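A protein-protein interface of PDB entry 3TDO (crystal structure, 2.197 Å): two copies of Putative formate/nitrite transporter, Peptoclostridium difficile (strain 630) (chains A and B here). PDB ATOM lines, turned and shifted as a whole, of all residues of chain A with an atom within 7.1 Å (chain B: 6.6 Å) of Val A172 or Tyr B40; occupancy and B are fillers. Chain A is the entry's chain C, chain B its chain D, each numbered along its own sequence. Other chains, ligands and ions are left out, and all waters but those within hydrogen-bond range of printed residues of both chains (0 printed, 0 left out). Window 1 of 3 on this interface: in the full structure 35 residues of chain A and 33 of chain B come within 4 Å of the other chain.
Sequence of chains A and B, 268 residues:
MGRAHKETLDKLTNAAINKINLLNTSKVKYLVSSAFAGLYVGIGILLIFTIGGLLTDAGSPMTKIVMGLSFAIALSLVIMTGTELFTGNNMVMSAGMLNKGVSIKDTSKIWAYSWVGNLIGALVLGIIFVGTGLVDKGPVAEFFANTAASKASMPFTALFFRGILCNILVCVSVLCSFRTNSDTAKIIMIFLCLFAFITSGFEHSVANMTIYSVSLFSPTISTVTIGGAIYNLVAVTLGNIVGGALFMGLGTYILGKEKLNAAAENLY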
ATOM      1  N   LEU A  75      21.679  12.618  11.923  1.00  0.00           N
ATOM      2  CA  LEU A  75      21.417  11.368  12.620  1.00  0.00           C
ATOM      3  C   LEU A  75      22.510  10.296  12.398  1.00  0.00           C
ATOM      4  O   LEU A  75      22.675   9.402  13.221  1.00  0.00           O
ATOM      5  CB  LEU A  75      20.008  10.841  12.273  1.00  0.00           C
ATOM      6  CG  LEU A  75      19.454   9.659  13.072  1.00  0.00           C
ATOM      7  CD1 LEU A  75      19.347   9.942  14.588  1.00  0.00           C
ATOM      8  CD2 LEU A  75      18.091   9.236  12.510  1.00  0.00           C
ATOM      9  N   MET A  91      10.540   6.712  20.678  1.00  0.00           N
ATOM     10  CA  MET A  91      10.241   5.328  20.322  1.00  0.00           C
ATOM     11  C   MET A  91      10.828   4.328  21.315  1.00  0.00           C
ATOM     12  O   MET A  91      10.128   3.446  21.804  1.00  0.00           O
ATOM     13  CB  MET A  91      10.760   4.979  18.921  1.00  0.00           C
ATOM     14  CG  MET A  91      10.647   3.480  18.587  1.00  0.00           C
ATOM     15  SD  MET A  91      11.324   2.974  16.974  1.00  0.00           S
ATOM     16  CE  MET A  91      13.077   3.308  17.196  1.00  0.00           C
ATOM     17  N   CYS A 166       7.850  13.839  10.989  1.00  0.00           N
ATOM     18  CA  CYS A 166       9.289  13.882  11.168  1.00  0.00           C
ATOM     19  C   CYS A 166       9.742  12.702  12.015  1.00  0.00           C
ATOM     20  O   CYS A 166      10.649  11.951  11.622  1.00  0.00           O
ATOM     21  CB  CYS A 166       9.718  15.188  11.834  1.00  0.00           C
ATOM     22  SG  CYS A 166      11.498  15.292  12.192  1.00  0.00           S
ATOM     23  N   ASN A 167       9.114  12.518  13.174  1.00  0.00           N
ATOM     24  CA  ASN A 167       9.622  11.503  14.093  1.00  0.00           C
ATOM     25  C   ASN A 167       9.310  10.059  13.691  1.00  0.00           C
ATOM     26  O   ASN A 167      10.049   9.133  14.038  1.00  0.00           O
ATOM     27  CB  ASN A 167       9.314  11.805  15.571  1.00  0.00           C
ATOM     28  CG  ASN A 167      10.504  11.490  16.481  1.00  0.00           C
ATOM     29  OD1 ASN A 167      11.633  11.345  16.006  1.00  0.00           O
ATOM     30  ND2 ASN A 167      10.255  11.376  17.781  1.00  0.00           N
ATOM     31  N   ILE A 168       8.247   9.867  12.926  1.00  0.00           N
ATOM     32  CA  ILE A 168       8.068   8.583  12.254  1.00  0.00           C
ATOM     33  C   ILE A 168       9.312   8.234  11.414  1.00  0.00           C
ATOM     34  O   ILE A 168       9.870   7.132  11.522  1.00  0.00           O
ATOM     35  CB  ILE A 168       6.799   8.579  11.394  1.00  0.00           C
ATOM     36  CG1 ILE A 168       5.570   8.495  12.305  1.00  0.00           C
ATOM     37  CG2 ILE A 168       6.815   7.409  10.421  1.00  0.00           C
ATOM     38  CD1 ILE A 168       4.260   8.730  11.589  1.00  0.00           C
ATOM     39  N   LEU A 169       9.771   9.199  10.625  1.00  0.00           N
ATOM     40  CA  LEU A 169      10.940   9.013   9.770  1.00  0.00           C
ATOM     41  C   LEU A 169      12.250   8.884  10.556  1.00  0.00           C
ATOM     42  O   LEU A 169      13.091   8.022  10.256  1.00  0.00           O
ATOM     43  CB  LEU A 169      11.046  10.154   8.767  1.00  0.00           C
ATOM     44  CG  LEU A 169      10.288   9.912   7.460  1.00  0.00           C
ATOM     45  CD1 LEU A 169       9.992  11.223   6.722  1.00  0.00           C
ATOM     46  CD2 LEU A 169      11.067   8.928   6.587  1.00  0.00           C
ATOM     47  N   VAL A 170      12.425   9.746  11.551  1.00  0.00           N
ATOM     48  CA  VAL A 170      13.619   9.692  12.378  1.00  0.00           C
ATOM     49  C   VAL A 170      13.652   8.396  13.194  1.00  0.00           C
ATOM     50  O   VAL A 170      14.683   7.728  13.249  1.00  0.00           O
ATOM     51  CB  VAL A 170      13.758  10.944  13.272  1.00  0.00           C
ATOM     52  CG1 VAL A 170      14.901  10.780  14.262  1.00  0.00           C
ATOM     53  CG2 VAL A 170      13.987  12.179  12.407  1.00  0.00           C
ATOM     54  N   CYS A 171      12.525   8.015  13.798  1.00  0.00           N
ATOM     55  CA  CYS A 171      12.515   6.795  14.598  1.00  0.00           C
ATOM     56  C   CYS A 171      12.578   5.529  13.745  1.00  0.00           C
ATOM     57  O   CYS A 171      13.206   4.548  14.161  1.00  0.00           O
ATOM     58  CB  CYS A 171      11.338   6.757  15.569  1.00  0.00           C
ATOM     59  SG  CYS A 171      11.499   7.941  16.920  1.00  0.00           S
ATOM     60  N   VAL A 172      11.953   5.543  12.562  1.00  0.00           N
ATOM     61  CA  VAL A 172      12.051   4.380  11.680  1.00  0.00           C
ATOM     62  C   VAL A 172      13.492   4.148  11.209  1.00  0.00           C
ATOM     63  O   VAL A 172      13.927   3.003  11.067  1.00  0.00           O
ATOM     64  CB  VAL A 172      11.085   4.437  10.476  1.00  0.00           C
ATOM     65  CG1 VAL A 172      11.732   5.156   9.288  1.00  0.00           C
ATOM     66  CG2 VAL A 172      10.661   3.030  10.085  1.00  0.00           C
ATOM     67  N   SER A 173      14.247   5.222  10.993  1.00  0.00           N
ATOM     68  CA  SER A 173      15.653   5.038  10.669  1.00  0.00           C
ATOM     69  C   SER A 173      16.404   4.429  11.845  1.00  0.00           C
ATOM     70  O   SER A 173      17.178   3.495  11.662  1.00  0.00           O
ATOM     71  CB  SER A 173      16.317   6.327  10.152  1.00  0.00           C
ATOM     72  OG  SER A 173      16.697   7.202  11.187  1.00  0.00           O
ATOM     73  N   VAL A 174      16.152   4.940  13.050  1.00  0.00           N
ATOM     74  CA  VAL A 174      16.644   4.319  14.278  1.00  0.00           C
ATOM     75  C   VAL A 174      16.247   2.846  14.360  1.00  0.00           C
ATOM     76  O   VAL A 174      17.087   1.993  14.658  1.00  0.00           O
ATOM     77  CB  VAL A 174      16.129   5.045  15.542  1.00  0.00           C
ATOM     78  CG1 VAL A 174      16.576   4.318  16.801  1.00  0.00           C
ATOM     79  CG2 VAL A 174      16.604   6.492  15.564  1.00  0.00           C
ATOM     80  N   LEU A 175      14.970   2.551  14.093  1.00  0.00           N
ATOM     81  CA  LEU A 175      14.476   1.165  14.056  1.00  0.00           C
ATOM     82  C   LEU A 175      15.273   0.287  13.076  1.00  0.00           C
ATOM     83  O   LEU A 175      15.702  -0.815  13.437  1.00  0.00           O
ATOM     84  CB  LEU A 175      12.978   1.116  13.699  1.00  0.00           C
ATOM     85  CG  LEU A 175      12.283  -0.258  13.731  1.00  0.00           C
ATOM     86  CD1 LEU A 175      12.458  -0.908  15.082  1.00  0.00           C
ATOM     87  CD2 LEU A 175      10.809  -0.150  13.400  1.00  0.00           C
ATOM     88  N   CYS A 176      15.470   0.766  11.842  1.00  0.00           N
ATOM     89  CA  CYS A 176      16.330   0.055  10.888  1.00  0.00           C
ATOM     90  C   CYS A 176      17.718  -0.229  11.458  1.00  0.00           C
ATOM     91  O   CYS A 176      18.321  -1.256  11.153  1.00  0.00           O
ATOM     92  CB  CYS A 176      16.468   0.820   9.551  1.00  0.00           C
ATOM     93  SG  CYS A 176      14.908   0.902   8.665  1.00  0.00           S
ATOM     94  N   SER A 177      18.227   0.685  12.272  1.00  0.00           N
ATOM     95  CA  SER A 177      19.564   0.514  12.822  1.00  0.00           C
ATOM     96  C   SER A 177      19.562  -0.674  13.796  1.00  0.00           C
ATOM     97  O   SER A 177      20.568  -1.367  13.946  1.00  0.00           O
ATOM     98  CB  SER A 177      20.031   1.786  13.530  1.00  0.00           C
ATOM     99  OG  SER A 177      19.582   1.802  14.875  1.00  0.00           O
ATOM    100  N   PHE A 178      18.419  -0.904  14.437  1.00  0.00           N
ATOM    101  CA  PHE A 178      18.242  -2.058  15.306  1.00  0.00           C
ATOM    102  C   PHE A 178      18.073  -3.352  14.520  1.00  0.00           C
ATOM    103  O   PHE A 178      18.327  -4.435  15.036  1.00  0.00           O
ATOM    104  CB  PHE A 178      17.029  -1.868  16.211  1.00  0.00           C
ATOM    105  CG  PHE A 178      17.309  -1.073  17.460  1.00  0.00           C
ATOM    106  CD1 PHE A 178      18.165  -1.555  18.430  1.00  0.00           C
ATOM    107  CD2 PHE A 178      16.697   0.153  17.667  1.00  0.00           C
ATOM    108  CE1 PHE A 178      18.411  -0.825  19.605  1.00  0.00           C
ATOM    109  CE2 PHE A 178      16.938   0.885  18.825  1.00  0.00           C
ATOM    110  CZ  PHE A 178      17.796   0.397  19.794  1.00  0.00           C
ATOM    111  N   MET A 189      20.030   3.972   5.312  1.00  0.00           N
ATOM    112  CA  MET A 189      18.623   4.135   5.665  1.00  0.00           C
ATOM    113  C   MET A 189      18.412   5.511   6.303  1.00  0.00           C
ATOM    114  O   MET A 189      17.365   6.130   6.137  1.00  0.00           O
ATOM    115  CB  MET A 189      18.119   3.005   6.588  1.00  0.00           C
ATOM    116  CG  MET A 189      18.057   1.651   5.897  1.00  0.00           C
ATOM    117  SD  MET A 189      17.123   1.761   4.327  1.00  0.00           S
ATOM    118  CE  MET A 189      15.474   2.147   4.936  1.00  0.00           C
ATOM    119  N   CYS A 193      15.832   8.440   5.013  1.00  0.00           N
ATOM    120  CA  CYS A 193      14.788   8.982   5.886  1.00  0.00           C
ATOM    121  C   CYS A 193      14.947  10.477   6.133  1.00  0.00           C
ATOM    122  O   CYS A 193      13.952  11.199   6.187  1.00  0.00           O
ATOM    123  CB  CYS A 193      14.710   8.223   7.221  1.00  0.00           C
ATOM    124  SG  CYS A 193      14.177   6.508   7.055  1.00  0.00           S
ATOM    125  N   MET A 248       5.546   4.661  16.398  1.00  0.00           N
ATOM    126  CA  MET A 248       6.650   3.724  16.251  1.00  0.00           C
ATOM    127  C   MET A 248       6.852   2.852  17.488  1.00  0.00           C
ATOM    128  O   MET A 248       7.203   1.674  17.372  1.00  0.00           O
ATOM    129  CB  MET A 248       7.949   4.462  15.896  1.00  0.00           C
ATOM    130  CG  MET A 248       7.876   5.241  14.615  1.00  0.00           C
ATOM    131  SD  MET A 248       7.440   4.240  13.172  1.00  0.00           S
ATOM    132  CE  MET A 248       8.596   2.882  13.321  1.00  0.00           C
ATOM    133  N   THR A 252       5.889  -1.050  17.081  1.00  0.00           N
ATOM    134  CA  THR A 252       6.913  -2.079  17.234  1.00  0.00           C
ATOM    135  C   THR A 252       6.595  -2.988  18.424  1.00  0.00           C
ATOM    136  O   THR A 252       6.896  -4.180  18.400  1.00  0.00           O
ATOM    137  CB  THR A 252       8.324  -1.473  17.397  1.00  0.00           C
ATOM    138  OG1 THR A 252       8.368  -0.663  18.580  1.00  0.00           O
ATOM    139  CG2 THR A 252       8.662  -0.619  16.211  1.00  0.00           C
ATOM    140  N   LEU A 255       3.898  -5.390  17.080  1.00  0.00           N
ATOM    141  CA  LEU A 255       4.493  -6.351  16.159  1.00  0.00           C
ATOM    142  C   LEU A 255       5.311  -7.436  16.870  1.00  0.00           C
ATOM    143  O   LEU A 255       5.334  -8.590  16.431  1.00  0.00           O
ATOM    144  CB  LEU A 255       5.390  -5.643  15.137  1.00  0.00           C
ATOM    145  CG  LEU A 255       4.777  -4.706  14.103  1.00  0.00           C
ATOM    146  CD1 LEU A 255       5.888  -4.194  13.143  1.00  0.00           C
ATOM    147  CD2 LEU A 255       3.651  -5.397  13.339  1.00  0.00           C
ATOM    148  N   SER B  33       1.204  -4.513  10.817  1.00  0.00           N
ATOM    149  CA  SER B  33       2.351  -4.664   9.930  1.00  0.00           C
ATOM    150  C   SER B  33       2.005  -4.152   8.526  1.00  0.00           C
ATOM    151  O   SER B  33       2.800  -3.442   7.903  1.00  0.00           O
ATOM    152  CB  SER B  33       2.805  -6.125   9.891  1.00  0.00           C
ATOM    153  OG  SER B  33       3.872  -6.323   8.985  1.00  0.00           O
ATOM    154  N   ALA B  35      -0.437  -1.994   7.744  1.00  0.00           N
ATOM    155  CA  ALA B  35      -0.601  -0.550   7.866  1.00  0.00           C
ATOM    156  C   ALA B  35       0.750   0.195   7.819  1.00  0.00           C
ATOM    157  O   ALA B  35       0.872   1.207   7.139  1.00  0.00           O
ATOM    158  CB  ALA B  35      -1.360  -0.219   9.152  1.00  0.00           C
ATOM    159  N   PHE B  36       1.758  -0.291   8.551  1.00  0.00           N
ATOM    160  CA  PHE B  36       3.095   0.321   8.507  1.00  0.00           C
ATOM    161  C   PHE B  36       3.633   0.361   7.081  1.00  0.00           C
ATOM    162  O   PHE B  36       4.144   1.389   6.619  1.00  0.00           O
ATOM    163  CB  PHE B  36       4.098  -0.463   9.368  1.00  0.00           C
ATOM    164  CG  PHE B  36       4.205   0.020  10.790  1.00  0.00           C
ATOM    165  CD1 PHE B  36       4.437   1.361  11.073  1.00  0.00           C
ATOM    166  CD2 PHE B  36       4.088  -0.877  11.848  1.00  0.00           C
ATOM    167  CE1 PHE B  36       4.548   1.802  12.388  1.00  0.00           C
ATOM    168  CE2 PHE B  36       4.198  -0.446  13.170  1.00  0.00           C
ATOM    169  CZ  PHE B  36       4.425   0.896  13.439  1.00  0.00           C
ATOM    170  N   ALA B  37       3.543  -0.779   6.401  1.00  0.00           N
ATOM    171  CA  ALA B  37       4.083  -0.903   5.053  1.00  0.00           C
ATOM    172  C   ALA B  37       3.361   0.040   4.087  1.00  0.00           C
ATOM    173  O   ALA B  37       3.980   0.610   3.195  1.00  0.00           O
ATOM    174  CB  ALA B  37       4.007  -2.346   4.567  1.00  0.00           C
ATOM    175  N   GLY B  38       2.056   0.212   4.274  1.00  0.00           N
ATOM    176  CA  GLY B  38       1.291   1.152   3.461  1.00  0.00           C
ATOM    177  C   GLY B  38       1.728   2.591   3.692  1.00  0.00           C
ATOM    178  O   GLY B  38       1.841   3.392   2.747  1.00  0.00           O
ATOM    179  N   LEU B  39       1.984   2.926   4.955  1.00  0.00           N
ATOM    180  CA  LEU B  39       2.448   4.267   5.294  1.00  0.00           C
ATOM    181  C   LEU B  39       3.902   4.549   4.834  1.00  0.00           C
ATOM    182  O   LEU B  39       4.191   5.626   4.299  1.00  0.00           O
ATOM    183  CB  LEU B  39       2.252   4.550   6.792  1.00  0.00           C
ATOM    184  CG  LEU B  39       2.764   5.927   7.216  1.00  0.00           C
ATOM    185  CD1 LEU B  39       1.972   6.487   8.392  1.00  0.00           C
ATOM    186  CD2 LEU B  39       4.260   5.840   7.528  1.00  0.00           C
ATOM    187  N   TYR B  40       4.790   3.573   5.008  1.00  0.00           N
ATOM    188  CA  TYR B  40       6.186   3.688   4.547  1.00  0.00           C
ATOM    189  C   TYR B  40       6.266   3.931   3.023  1.00  0.00           C
ATOM    190  O   TYR B  40       7.094   4.723   2.536  1.00  0.00           O
ATOM    191  CB  TYR B  40       6.971   2.414   4.898  1.00  0.00           C
ATOM    192  CG  TYR B  40       7.190   2.142   6.384  1.00  0.00           C
ATOM    193  CD1 TYR B  40       7.189   3.168   7.310  1.00  0.00           C
ATOM    194  CD2 TYR B  40       7.398   0.844   6.849  1.00  0.00           C
ATOM    195  CE1 TYR B  40       7.393   2.914   8.657  1.00  0.00           C
ATOM    196  CE2 TYR B  40       7.602   0.582   8.186  1.00  0.00           C
ATOM    197  CZ  TYR B  40       7.597   1.626   9.088  1.00  0.00           C
ATOM    198  OH  TYR B  40       7.801   1.384  10.428  1.00  0.00           O
ATOM    199  N   VAL B  41       5.415   3.239   2.267  1.00  0.00           N
ATOM    200  CA  VAL B  41       5.353   3.448   0.817  1.00  0.00           C
ATOM    201  C   VAL B  41       4.799   4.848   0.504  1.00  0.00           C
ATOM    202  O   VAL B  41       5.319   5.551  -0.365  1.00  0.00           O
ATOM    203  CB  VAL B  41       4.501   2.342   0.107  1.00  0.00           C
ATOM    204  CG1 VAL B  41       4.137   2.741  -1.295  1.00  0.00           C
ATOM    205  CG2 VAL B  41       5.227   0.977   0.107  1.00  0.00           C
ATOM    206  N   GLY B  42       3.759   5.259   1.228  1.00  0.00           N
ATOM    207  CA  GLY B  42       3.165   6.580   1.051  1.00  0.00           C
ATOM    208  C   GLY B  42       4.189   7.672   1.327  1.00  0.00           C
ATOM    209  O   GLY B  42       4.173   8.733   0.703  1.00  0.00           O
ATOM    210  N   ILE B  43       5.099   7.389   2.253  1.00  0.00           N
ATOM    211  CA  ILE B  43       6.163   8.312   2.605  1.00  0.00           C
ATOM    212  C   ILE B  43       7.032   8.570   1.371  1.00  0.00           C
ATOM    213  O   ILE B  43       7.390   9.707   1.087  1.00  0.00           O
ATOM    214  CB  ILE B  43       6.996   7.792   3.813  1.00  0.00           C
ATOM    215  CG1 ILE B  43       6.301   8.154   5.120  1.00  0.00           C
ATOM    216  CG2 ILE B  43       8.413   8.396   3.818  1.00  0.00           C
ATOM    217  CD1 ILE B  43       6.937   7.521   6.356  1.00  0.00           C
ATOM    218  N   GLY B  44       7.331   7.525   0.606  1.00  0.00           N
ATOM    219  CA  GLY B  44       8.062   7.734  -0.633  1.00  0.00           C
ATOM    220  C   GLY B  44       7.313   8.695  -1.543  1.00  0.00           C
ATOM    221  O   GLY B  44       7.885   9.621  -2.124  1.00  0.00           O
ATOM    222  N   ILE B  45       6.012   8.475  -1.668  1.00  0.00           N
ATOM    223  CA  ILE B  45       5.159   9.315  -2.514  1.00  0.00           C
ATOM    224  C   ILE B  45       5.149  10.785  -2.084  1.00  0.00           C
ATOM    225  O   ILE B  45       5.176  11.669  -2.923  1.00  0.00           O
ATOM    226  CB  ILE B  45       3.691   8.814  -2.502  1.00  0.00           C
ATOM    227  CG1 ILE B  45       3.575   7.480  -3.246  1.00  0.00           C
ATOM    228  CG2 ILE B  45       2.768   9.890  -3.118  1.00  0.00           C
ATOM    229  CD1 ILE B  45       3.703   7.651  -4.771  1.00  0.00           C
ATOM    230  N   ILE B  73      13.228   4.770  -0.852  1.00  0.00           N
ATOM    231  CA  ILE B  73      12.842   4.653   0.551  1.00  0.00           C
ATOM    232  C   ILE B  73      11.556   3.856   0.733  1.00  0.00           C
ATOM    233  O   ILE B  73      11.357   3.182   1.750  1.00  0.00           O
ATOM    234  CB  ILE B  73      12.691   6.053   1.211  1.00  0.00           C
ATOM    235  CG1 ILE B  73      12.411   5.919   2.707  1.00  0.00           C
ATOM    236  CG2 ILE B  73      11.601   6.853   0.518  1.00  0.00           C
ATOM    237  CD1 ILE B  73      12.319   7.249   3.442  1.00  0.00           C
ATOM    238  N   ALA B  74      10.681   3.932  -0.253  1.00  0.00           N
ATOM    239  CA  ALA B  74       9.377   3.287  -0.133  1.00  0.00           C
ATOM    240  C   ALA B  74       9.535   1.809   0.236  1.00  0.00           C
ATOM    241  O   ALA B  74       9.132   1.390   1.312  1.00  0.00           O
ATOM    242  CB  ALA B  74       8.582   3.445  -1.404  1.00  0.00           C
ATOM    243  N   LEU B  75      10.129   1.040  -0.670  1.00  0.00           N
ATOM    244  CA  LEU B  75      10.349  -0.384  -0.456  1.00  0.00           C
ATOM    245  C   LEU B  75      11.527  -0.698   0.471  1.00  0.00           C
ATOM    246  O   LEU B  75      11.538  -1.751   1.125  1.00  0.00           O
ATOM    247  CB  LEU B  75      10.512  -1.086  -1.811  1.00  0.00           C
ATOM    248  CG  LEU B  75      10.348  -2.609  -1.887  1.00  0.00           C
ATOM    249  CD1 LEU B  75       9.076  -3.134  -1.187  1.00  0.00           C
ATOM    250  CD2 LEU B  75      10.402  -3.068  -3.343  1.00  0.00           C
ATOM    251  N   LEU B  77      12.230   0.847   3.226  1.00  0.00           N
ATOM    252  CA  LEU B  77      11.689   0.862   4.575  1.00  0.00           C
ATOM    253  C   LEU B  77      10.886  -0.416   4.810  1.00  0.00           C
ATOM    254  O   LEU B  77      10.966  -1.027   5.867  1.00  0.00           O
ATOM    255  CB  LEU B  77      10.770   2.064   4.768  1.00  0.00           C
ATOM    256  CG  LEU B  77      11.407   3.399   5.132  1.00  0.00           C
ATOM    257  CD1 LEU B  77      10.292   4.445   5.364  1.00  0.00           C
ATOM    258  CD2 LEU B  77      12.275   3.238   6.367  1.00  0.00           C
ATOM    259  N   VAL B  78      10.114  -0.825   3.808  1.00  0.00           N
ATOM    260  CA  VAL B  78       9.324  -2.049   3.949  1.00  0.00           C
ATOM    261  C   VAL B  78      10.195  -3.281   4.197  1.00  0.00           C
ATOM    262  O   VAL B  78       9.945  -4.062   5.109  1.00  0.00           O
ATOM    263  CB  VAL B  78       8.398  -2.267   2.734  1.00  0.00           C
ATOM    264  CG1 VAL B  78       7.966  -3.739   2.617  1.00  0.00           C
ATOM    265  CG2 VAL B  78       7.191  -1.362   2.839  1.00  0.00           C
ATOM    266  N   THR B  81      12.155  -3.096   7.685  1.00  0.00           N
ATOM    267  CA  THR B  81      11.280  -3.268   8.870  1.00  0.00           C
ATOM    268  C   THR B  81      10.554  -4.627   8.935  1.00  0.00           C
ATOM    269  O   THR B  81       9.916  -4.978   9.951  1.00  0.00           O
ATOM    270  CB  THR B  81      10.232  -2.139   8.969  1.00  0.00           C
ATOM    271  OG1 THR B  81       9.434  -2.105   7.768  1.00  0.00           O
ATOM    272  CG2 THR B  81      10.929  -0.798   9.141  1.00  0.00           C
ATOM    273  N   THR B  83       7.961  -5.515   7.201  1.00  0.00           N
ATOM    274  CA  THR B  83       6.513  -5.329   7.245  1.00  0.00           C
ATOM    275  C   THR B  83       5.808  -5.921   6.010  1.00  0.00           C
ATOM    276  O   THR B  83       6.463  -6.332   5.047  1.00  0.00           O
ATOM    277  CB  THR B  83       6.141  -3.842   7.502  1.00  0.00           C
ATOM    278  OG1 THR B  83       6.969  -3.000   6.701  1.00  0.00           O
ATOM    279  CG2 THR B  83       6.393  -3.475   8.979  1.00  0.00           C
ATOM    280  N   GLY B 121      -2.930   2.134   6.230  1.00  0.00           N
ATOM    281  CA  GLY B 121      -1.703   2.894   6.395  1.00  0.00           C
ATOM    282  C   GLY B 121      -1.706   4.170   5.558  1.00  0.00           C
ATOM    283  O   GLY B 121      -1.337   5.245   6.035  1.00  0.00           O
ATOM    284  N   LEU B 125      -1.668   8.106   6.849  1.00  0.00           N
ATOM    285  CA  LEU B 125      -0.656   9.011   6.307  1.00  0.00           C
ATOM    286  C   LEU B 125      -1.289  10.204   5.572  1.00  0.00           C
ATOM    287  O   LEU B 125      -0.929  11.358   5.820  1.00  0.00           O
ATOM    288  CB  LEU B 125       0.313   8.263   5.389  1.00  0.00           C
ATOM    289  CG  LEU B 125       1.436   9.118   4.781  1.00  0.00           C
ATOM    290  CD1 LEU B 125       2.335   9.713   5.864  1.00  0.00           C
ATOM    291  CD2 LEU B 125       2.262   8.305   3.797  1.00  0.00           C
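Of the 21 printed residues of chain B, 7 touch a printed residue of chain A.
Hydrophobic or aromatic side chains of chain B that line the printed part of chain A: Phe B36, Tyr B40, Ile B43, Ile B73 and Leu B77.
Printed residues of chain A that touch a printed residue of chain B: Leu A169, Val A172, Met A189, Cys A193, Met A248 and Leu A255.
Hydrophobic or aromatic side chains of chain A that line the printed part of chain B: Leu A169, Val A172, Met A189, Met A248 and Leu A255.
Along chain A the printed residues that touch a printed residue of chain B span positions 169 to 255.
Among the printed residues, 12 pairs touch across the chains.
Among the printed residues, no Asp or Glu carboxylate lies within 4 Å of a Lys or Arg side-chain nitrogen of the other chain.
Among the printed residues, merely in contact across the chains: Val A172 with Tyr B40 (3.3 Å), Met A248 with Tyr B40 (3.4 Å), Val A172 with Leu B77 (3.5 Å), Leu A255 with Ser B33 (3.6 Å), Met A189 with Leu B77 (3.7 Å), Leu A169 with Ile B73 (3.8 Å), Cys A193 with Leu B77 (3.8 Å), Met A248 with Phe B36 (3.9 Å), Leu A169 with Ile B43 (3.9 Å), Cys A193 with Ile B73 (3.9 Å), Val A172 with Thr B81 (3.95 Å) and Leu A255 with Phe B36 (3.99 Å).
O of Leu A169 sits close to SG of Cys A193 (3.7 Å).
The side-chain sulfur (SG) of Cys A176 sits at hydrogen-bond distance from the backbone carbonyl oxygen (O) of Val A172, 3.3 Å away.
The backbone carbonyl oxygen of Met A189 sits at hydrogen-bond distance from the side-chain sulfur of Cys A193 (3.3 Å).
O of Met A248 is in hydrogen-bond range of OG1 of Thr A252, at 2.9 Å.
The backbone carbonyl oxygen (O) of Leu B77 lies within hydrogen-bond range of the side-chain hydroxyl (OG1) of Thr B81 (2.7 Å).
The side-chain hydroxyl of Thr B81 lies within hydrogen-bond range of the side-chain hydroxyl of Thr B83 (2.8 Å).
Printed residues of chain B within 4 Å of Val A172: Tyr B40, Leu B77 and Thr B81.
Of the printed residues of chain B, Leu A255 touches Ser B33 and Phe B36.
Of the printed residues of chain A, Ile B73 touches Leu A169 (3.8 Å) and Cys A193 (3.9 Å).
Of the printed residues of chain A, Thr B81 touches Val A172.
The nearest residue of chain A that does not touch Tyr B40 is Leu A175 (4.5 Å).
The nearest printed residue of chain B that does not touch Met A248 is Thr B81 (6.0 Å).
1 position is printed for both chains.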
